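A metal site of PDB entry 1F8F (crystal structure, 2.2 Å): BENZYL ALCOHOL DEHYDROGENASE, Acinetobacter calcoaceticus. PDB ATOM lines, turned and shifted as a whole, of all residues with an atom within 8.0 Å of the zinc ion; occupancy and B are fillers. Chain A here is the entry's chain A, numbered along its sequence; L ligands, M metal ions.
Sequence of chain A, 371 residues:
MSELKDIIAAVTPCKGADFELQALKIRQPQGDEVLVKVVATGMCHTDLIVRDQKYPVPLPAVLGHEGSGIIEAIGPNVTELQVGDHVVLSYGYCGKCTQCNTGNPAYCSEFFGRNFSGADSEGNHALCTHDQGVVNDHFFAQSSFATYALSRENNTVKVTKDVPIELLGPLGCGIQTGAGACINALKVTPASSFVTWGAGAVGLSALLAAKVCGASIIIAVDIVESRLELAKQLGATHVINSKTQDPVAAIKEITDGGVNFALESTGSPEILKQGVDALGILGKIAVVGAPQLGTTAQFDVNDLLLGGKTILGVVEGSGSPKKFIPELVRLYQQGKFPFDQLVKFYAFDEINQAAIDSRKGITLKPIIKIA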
ATOM      1  N   GLY A  42     -19.689 -25.123  23.700  1.00  0.00           N
ATOM      2  CA  GLY A  42     -19.699 -23.677  23.449  1.00  0.00           C
ATOM      3  C   GLY A  42     -19.862 -22.828  24.692  1.00  0.00           C
ATOM      4  O   GLY A  42     -20.375 -23.293  25.708  1.00  0.00           O
ATOM      5  N   MET A  43     -19.462 -21.560  24.649  1.00  0.00           N
ATOM      6  CA  MET A  43     -19.589 -20.613  25.737  1.00  0.00           C
ATOM      7  C   MET A  43     -20.549 -19.490  25.325  1.00  0.00           C
ATOM      8  O   MET A  43     -20.472 -18.918  24.252  1.00  0.00           O
ATOM      9  CB  MET A  43     -18.298 -19.899  26.162  1.00  0.00           C
ATOM     10  CG  MET A  43     -18.513 -19.068  27.433  1.00  0.00           C
ATOM     11  SD  MET A  43     -16.993 -18.089  27.802  1.00  0.00           S
ATOM     12  CE  MET A  43     -15.929 -19.412  28.363  1.00  0.00           C
ATOM     13  N   CYS A  44     -21.455 -19.178  26.223  1.00  0.00           N
ATOM     14  CA  CYS A  44     -22.539 -18.222  26.006  1.00  0.00           C
ATOM     15  C   CYS A  44     -22.626 -17.263  27.168  1.00  0.00           C
ATOM     16  O   CYS A  44     -22.379 -17.503  28.344  1.00  0.00           O
ATOM     17  CB  CYS A  44     -23.822 -19.028  25.752  1.00  0.00           C
ATOM     18  SG  CYS A  44     -25.412 -18.241  26.011  1.00  0.00           S
ATOM     19  N   HIS A  45     -23.077 -16.077  26.857  1.00  0.00           N
ATOM     20  CA  HIS A  45     -23.300 -14.941  27.727  1.00  0.00           C
ATOM     21  C   HIS A  45     -23.974 -15.343  29.018  1.00  0.00           C
ATOM     22  O   HIS A  45     -23.607 -14.983  30.138  1.00  0.00           O
ATOM     23  CB  HIS A  45     -24.089 -13.903  26.888  1.00  0.00           C
ATOM     24  CG  HIS A  45     -24.094 -12.592  27.633  1.00  0.00           C
ATOM     25  ND1 HIS A  45     -25.247 -11.958  28.028  1.00  0.00           N
ATOM     26  CD2 HIS A  45     -23.045 -11.859  28.095  1.00  0.00           C
ATOM     27  CE1 HIS A  45     -24.931 -10.861  28.690  1.00  0.00           C
ATOM     28  NE2 HIS A  45     -23.607 -10.776  28.738  1.00  0.00           N
ATOM     29  N   THR A  46     -24.991 -16.201  28.892  1.00  0.00           N
ATOM     30  CA  THR A  46     -25.718 -16.781  29.966  1.00  0.00           C
ATOM     31  C   THR A  46     -24.860 -17.532  30.958  1.00  0.00           C
ATOM     32  O   THR A  46     -25.205 -17.489  32.165  1.00  0.00           O
ATOM     33  CB  THR A  46     -26.886 -17.658  29.438  1.00  0.00           C
ATOM     34  OG1 THR A  46     -27.689 -16.865  28.531  1.00  0.00           O
ATOM     35  CG2 THR A  46     -27.742 -18.090  30.603  1.00  0.00           C
ATOM     36  N   ASP A  47     -23.757 -18.183  30.574  1.00  0.00           N
ATOM     37  CA  ASP A  47     -22.935 -18.844  31.611  1.00  0.00           C
ATOM     38  C   ASP A  47     -22.363 -17.762  32.551  1.00  0.00           C
ATOM     39  O   ASP A  47     -22.251 -17.902  33.762  1.00  0.00           O
ATOM     40  CB  ASP A  47     -21.832 -19.715  31.061  1.00  0.00           C
ATOM     41  CG  ASP A  47     -22.098 -20.926  30.249  1.00  0.00           C
ATOM     42  OD1 ASP A  47     -22.024 -22.121  30.663  1.00  0.00           O
ATOM     43  OD2 ASP A  47     -22.417 -20.765  29.039  1.00  0.00           O
ATOM     44  N   HIS A  65     -23.471 -25.113  28.692  1.00  0.00           N
ATOM     45  CA  HIS A  65     -24.801 -25.510  28.270  1.00  0.00           C
ATOM     46  C   HIS A  65     -24.832 -25.632  26.743  1.00  0.00           C
ATOM     47  O   HIS A  65     -25.896 -25.554  26.144  1.00  0.00           O
ATOM     48  CB  HIS A  65     -25.900 -24.618  28.809  1.00  0.00           C
ATOM     49  CG  HIS A  65     -25.950 -23.214  28.314  1.00  0.00           C
ATOM     50  ND1 HIS A  65     -25.105 -22.249  28.844  1.00  0.00           N
ATOM     51  CD2 HIS A  65     -26.731 -22.605  27.407  1.00  0.00           C
ATOM     52  CE1 HIS A  65     -25.343 -21.074  28.254  1.00  0.00           C
ATOM     53  NE2 HIS A  65     -26.325 -21.266  27.362  1.00  0.00           N
ATOM     54  N   GLU A  66     -23.611 -25.677  26.176  1.00  0.00           N
ATOM     55  CA  GLU A  66     -23.557 -25.869  24.715  1.00  0.00           C
ATOM     56  C   GLU A  66     -22.693 -27.051  24.323  1.00  0.00           C
ATOM     57  O   GLU A  66     -21.822 -26.961  23.443  1.00  0.00           O
ATOM     58  CB  GLU A  66     -23.141 -24.577  24.018  1.00  0.00           C
ATOM     59  CG  GLU A  66     -24.127 -23.411  24.145  1.00  0.00           C
ATOM     60  CD  GLU A  66     -23.696 -22.179  23.366  1.00  0.00           C
ATOM     61  OE1 GLU A  66     -22.536 -21.977  22.982  1.00  0.00           O
ATOM     62  OE2 GLU A  66     -24.552 -21.325  23.053  1.00  0.00           O
ATOM     63  N   PHE A 139     -27.357 -28.375  34.965  1.00  0.00           N
ATOM     64  CA  PHE A 139     -27.496 -27.016  34.469  1.00  0.00           C
ATOM     65  C   PHE A 139     -27.840 -27.037  32.987  1.00  0.00           C
ATOM     66  O   PHE A 139     -27.136 -27.563  32.138  1.00  0.00           O
ATOM     67  CB  PHE A 139     -26.214 -26.226  34.739  1.00  0.00           C
ATOM     68  CG  PHE A 139     -26.264 -24.813  34.203  1.00  0.00           C
ATOM     69  CD1 PHE A 139     -27.197 -23.921  34.692  1.00  0.00           C
ATOM     70  CD2 PHE A 139     -25.356 -24.387  33.236  1.00  0.00           C
ATOM     71  CE1 PHE A 139     -27.233 -22.631  34.251  1.00  0.00           C
ATOM     72  CE2 PHE A 139     -25.415 -23.083  32.776  1.00  0.00           C
ATOM     73  CZ  PHE A 139     -26.362 -22.199  33.280  1.00  0.00           C
ATOM     74  N   PHE A 140     -29.038 -26.563  32.661  1.00  0.00           N
ATOM     75  CA  PHE A 140     -29.655 -26.656  31.361  1.00  0.00           C
ATOM     76  C   PHE A 140     -29.719 -28.169  31.054  1.00  0.00           C
ATOM     77  O   PHE A 140     -29.461 -28.580  29.944  1.00  0.00           O
ATOM     78  CB  PHE A 140     -28.945 -25.870  30.275  1.00  0.00           C
ATOM     79  CG  PHE A 140     -29.280 -24.385  30.204  1.00  0.00           C
ATOM     80  CD1 PHE A 140     -28.984 -23.440  31.148  1.00  0.00           C
ATOM     81  CD2 PHE A 140     -29.959 -24.004  29.026  1.00  0.00           C
ATOM     82  CE1 PHE A 140     -29.357 -22.135  30.949  1.00  0.00           C
ATOM     83  CE2 PHE A 140     -30.321 -22.698  28.805  1.00  0.00           C
ATOM     84  CZ  PHE A 140     -30.020 -21.739  29.779  1.00  0.00           C
ATOM     85  N   PRO A 170     -22.654 -25.300  20.049  1.00  0.00           N
ATOM     86  CA  PRO A 170     -23.337 -24.013  20.052  1.00  0.00           C
ATOM     87  C   PRO A 170     -24.703 -24.021  19.415  1.00  0.00           C
ATOM     88  O   PRO A 170     -25.596 -23.220  19.718  1.00  0.00           O
ATOM     89  CB  PRO A 170     -22.363 -23.103  19.275  1.00  0.00           C
ATOM     90  CG  PRO A 170     -21.010 -23.701  19.642  1.00  0.00           C
ATOM     91  CD  PRO A 170     -21.281 -25.198  19.481  1.00  0.00           C
ATOM     92  N   GLY A 172     -26.940 -26.080  20.236  1.00  0.00           N
ATOM     93  CA  GLY A 172     -27.931 -26.358  21.316  1.00  0.00           C
ATOM     94  C   GLY A 172     -28.420 -25.106  22.067  1.00  0.00           C
ATOM     95  O   GLY A 172     -29.219 -25.231  23.013  1.00  0.00           O
ATOM     96  N   CYS A 173     -27.934 -23.904  21.758  1.00  0.00           N
ATOM     97  CA  CYS A 173     -28.366 -22.688  22.380  1.00  0.00           C
ATOM     98  C   CYS A 173     -28.280 -21.442  21.493  1.00  0.00           C
ATOM     99  O   CYS A 173     -29.299 -21.051  20.922  1.00  0.00           O
ATOM    100  CB  CYS A 173     -27.659 -22.280  23.686  1.00  0.00           C
ATOM    101  SG  CYS A 173     -28.444 -20.849  24.499  1.00  0.00           S
ATOM    102  N   GLY A 174     -27.156 -20.718  21.509  1.00  0.00           N
ATOM    103  CA  GLY A 174     -27.122 -19.437  20.780  1.00  0.00           C
ATOM    104  C   GLY A 174     -27.432 -19.442  19.279  1.00  0.00           C
ATOM    105  O   GLY A 174     -28.082 -18.476  18.791  1.00  0.00           O
ATOM    106  N   ILE A 175     -26.977 -20.403  18.495  1.00  0.00           N
ATOM    107  CA  ILE A 175     -27.250 -20.466  17.055  1.00  0.00           C
ATOM    108  C   ILE A 175     -28.711 -20.787  16.754  1.00  0.00           C
ATOM    109  O   ILE A 175     -29.325 -20.071  15.975  1.00  0.00           O
ATOM    110  CB  ILE A 175     -26.281 -21.406  16.336  1.00  0.00           C
ATOM    111  CG1 ILE A 175     -24.857 -21.301  16.902  1.00  0.00           C
ATOM    112  CG2 ILE A 175     -26.251 -21.129  14.815  1.00  0.00           C
ATOM    113  CD1 ILE A 175     -24.170 -19.935  16.768  1.00  0.00           C
ATOM    114  N   THR A 177     -31.109 -20.169  18.770  1.00  0.00           N
ATOM    115  CA  THR A 177     -31.905 -19.075  19.300  1.00  0.00           C
ATOM    116  C   THR A 177     -32.087 -17.981  18.242  1.00  0.00           C
ATOM    117  O   THR A 177     -33.172 -17.468  17.960  1.00  0.00           O
ATOM    118  CB  THR A 177     -31.314 -18.437  20.585  1.00  0.00           C
ATOM    119  OG1 THR A 177     -31.341 -19.328  21.697  1.00  0.00           O
ATOM    120  CG2 THR A 177     -32.118 -17.198  21.009  1.00  0.00           C
ATOM    121  N   VAL A 202     -25.788 -14.397  18.541  1.00  0.00           N
ATOM    122  CA  VAL A 202     -27.218 -14.574  18.395  1.00  0.00           C
ATOM    123  C   VAL A 202     -27.699 -13.760  17.182  1.00  0.00           C
ATOM    124  O   VAL A 202     -28.297 -14.277  16.250  1.00  0.00           O
ATOM    125  CB  VAL A 202     -28.003 -14.129  19.650  1.00  0.00           C
ATOM    126  CG1 VAL A 202     -29.517 -14.162  19.344  1.00  0.00           C
ATOM    127  CG2 VAL A 202     -27.748 -14.981  20.907  1.00  0.00           C
ATOM    128  N   GLU A 316     -35.225 -19.568  23.149  1.00  0.00           N
ATOM    129  CA  GLU A 316     -34.519 -20.542  22.364  1.00  0.00           C
ATOM    130  C   GLU A 316     -35.046 -20.727  20.948  1.00  0.00           C
ATOM    131  O   GLU A 316     -34.879 -21.789  20.336  1.00  0.00           O
ATOM    132  CB  GLU A 316     -34.537 -21.914  23.092  1.00  0.00           C
ATOM    133  CG  GLU A 316     -33.929 -21.853  24.477  1.00  0.00           C
ATOM    134  CD  GLU A 316     -32.407 -22.076  24.419  1.00  0.00           C
ATOM    135  OE1 GLU A 316     -31.831 -22.428  23.354  1.00  0.00           O
ATOM    136  OE2 GLU A 316     -31.764 -21.908  25.441  1.00  0.00           O
ATOM    137  N   LYS A 365     -18.169 -16.336  19.272  1.00  0.00           N
ATOM    138  CA  LYS A 365     -18.552 -17.610  19.887  1.00  0.00           C
ATOM    139  C   LYS A 365     -17.373 -18.498  20.264  1.00  0.00           C
ATOM    140  O   LYS A 365     -16.953 -19.333  19.469  1.00  0.00           O
ATOM    141  CB  LYS A 365     -19.535 -18.366  18.937  1.00  0.00           C
ATOM    142  CG  LYS A 365     -19.863 -19.786  19.325  1.00  0.00           C
ATOM    143  CD  LYS A 365     -20.519 -19.852  20.725  1.00  0.00           C
ATOM    144  CE  LYS A 365     -21.864 -19.155  20.776  1.00  0.00           C
ATOM    145  NZ  LYS A 365     -22.467 -19.170  22.172  1.00  0.00           N
HETATM  146  C1  LIG L   1     -30.305 -19.274  27.358  1.00  0.00           C
HETATM  147  C2  LIG L   1     -31.394 -18.476  27.947  1.00  0.00           C
HETATM  148  O1  LIG L   1     -29.014 -18.688  27.208  1.00  0.00           O
HETATM  149  P1  LG2 L   2     -22.960 -11.209  22.613  1.00  0.00           P
HETATM  150  O1  LG2 L   2     -22.139 -12.091  21.734  1.00  0.00           O
HETATM  151  O2  LG2 L   2     -22.285 -10.520  23.723  1.00  0.00           O
HETATM  152  O3  LG2 L   2     -23.838 -10.222  21.733  1.00  0.00           O
HETATM  153  C1  LG2 L   2     -24.623  -9.051  22.081  1.00  0.00           C
HETATM  154  C2  LG2 L   2     -24.180  -7.846  21.279  1.00  0.00           C
HETATM  155  O4  LG2 L   2     -24.906  -6.662  21.756  1.00  0.00           O
HETATM  156  C3  LG2 L   2     -22.684  -7.472  21.335  1.00  0.00           C
HETATM  157  O5  LG2 L   2     -22.056  -7.596  20.075  1.00  0.00           O
HETATM  158  C4  LG2 L   2     -22.634  -6.007  21.778  1.00  0.00           C
HETATM  159  O6  LG2 L   2     -21.700  -5.192  21.062  1.00  0.00           O
HETATM  160  C5  LG2 L   2     -24.070  -5.549  21.494  1.00  0.00           C
HETATM  161  N1  LG2 L   2     -24.524  -4.418  22.297  1.00  0.00           N
HETATM  162  C6  LG2 L   2     -24.527  -4.284  23.657  1.00  0.00           C
HETATM  163  N2  LG2 L   2     -25.018  -3.112  24.062  1.00  0.00           N
HETATM  164  C7  LG2 L   2     -25.334  -2.463  22.883  1.00  0.00           C
HETATM  165  C8  LG2 L   2     -25.879  -1.190  22.617  1.00  0.00           C
HETATM  166  N3  LG2 L   2     -26.236  -0.294  23.532  1.00  0.00           N
HETATM  167  N4  LG2 L   2     -26.073  -0.859  21.318  1.00  0.00           N
HETATM  168  C9  LG2 L   2     -25.718  -1.753  20.339  1.00  0.00           C
HETATM  169  N5  LG2 L   2     -25.207  -2.945  20.488  1.00  0.00           N
HETATM  170  C10 LG2 L   2     -25.026  -3.241  21.788  1.00  0.00           C
HETATM  171  O7  LG2 L   2     -24.140 -12.156  23.220  1.00  0.00           O
HETATM  172  P2  LG2 L   2     -24.903 -13.313  22.424  1.00  0.00           P
HETATM  173  O8  LG2 L   2     -25.193 -12.904  21.041  1.00  0.00           O
HETATM  174  O9  LG2 L   2     -24.136 -14.559  22.536  1.00  0.00           O
HETATM  175  O10 LG2 L   2     -26.248 -13.378  23.339  1.00  0.00           O
HETATM  176  C11 LG2 L   2     -27.272 -12.385  23.130  1.00  0.00           C
HETATM  177  C12 LG2 L   2     -28.236 -12.232  24.260  1.00  0.00           C
HETATM  178  O11 LG2 L   2     -29.347 -13.179  24.183  1.00  0.00           O
HETATM  179  C13 LG2 L   2     -27.797 -12.186  25.730  1.00  0.00           C
HETATM  180  O12 LG2 L   2     -28.734 -11.366  26.454  1.00  0.00           O
HETATM  181  C14 LG2 L   2     -28.075 -13.647  26.122  1.00  0.00           C
HETATM  182  O13 LG2 L   2     -28.047 -13.881  27.523  1.00  0.00           O
HETATM  183  C15 LG2 L   2     -29.479 -13.721  25.513  1.00  0.00           C
HETATM  184  N6  LG2 L   2     -29.871 -15.107  25.308  1.00  0.00           N
HETATM  185  C16 LG2 L   2     -31.211 -15.341  25.257  1.00  0.00           C
HETATM  186  C17 LG2 L   2     -31.634 -16.627  25.006  1.00  0.00           C
HETATM  187  C18 LG2 L   2     -33.149 -17.028  24.911  1.00  0.00           C
HETATM  188  O14 LG2 L   2     -33.458 -18.200  24.713  1.00  0.00           O
HETATM  189  N7  LG2 L   2     -34.036 -15.973  25.063  1.00  0.00           N
HETATM  190  C19 LG2 L   2     -30.696 -17.677  24.762  1.00  0.00           C
HETATM  191  C20 LG2 L   2     -29.467 -17.173  24.281  1.00  0.00           C
HETATM  192  C21 LG2 L   2     -28.977 -15.912  24.527  1.00  0.00           C
HETATM  193 ZN    ZN M   1     -27.258 -19.795  25.972  1.00  0.00          ZN
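ND1 of His 65 lies close to OD2 of Asp 47 (3.1 Å).
O of Cys 173 is in hydrogen-bond range of OG1 of Thr 177.
SG of Cys 173 lies close to OE2 of Glu 316 (3.6 Å).
The backbone NH (N) of Cys 44 sits at hydrogen-bond distance from the side-chain carboxylate (OD2) of Asp 47 (3.4 Å).
SG of Cys 44 lies close to N of Thr 46.
An oxygen (O14) of LG2 L2 sits at hydrogen-bond distance from the backbone NH of Glu 316 (2.7 Å).
The backbone NH (N) of Val 202 lies within hydrogen-bond range of an oxygen (O8) of LG2 L2 (3.0 Å).
An oxygen (O13) of LG2 L2 lies within hydrogen-bond range of the side-chain hydroxyl (OG1) of Thr 46 (3.2 Å).
ND1 of His 45 lies within hydrogen-bond range of O13 of LG2 L2 (3.4 Å).
Thr 46 touches the zinc ion (OG1 to ZN, 3.9 Å).
Within 4 Å of the zinc ion: Cys 44, Thr 46, His 65 and Cys 173.
The nearest printed residue that does not touch the zinc ion is Glu 66 (4.3 Å).
The zinc ion is bound by SG of Cys 173 (2.2 Å), NE2 of His 65 (2.2 Å), SG of Cys 44 (2.4 Å) and O1 of LIG L1 (2.4 Å).
The zinc ion has four donor atoms within binding distance.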
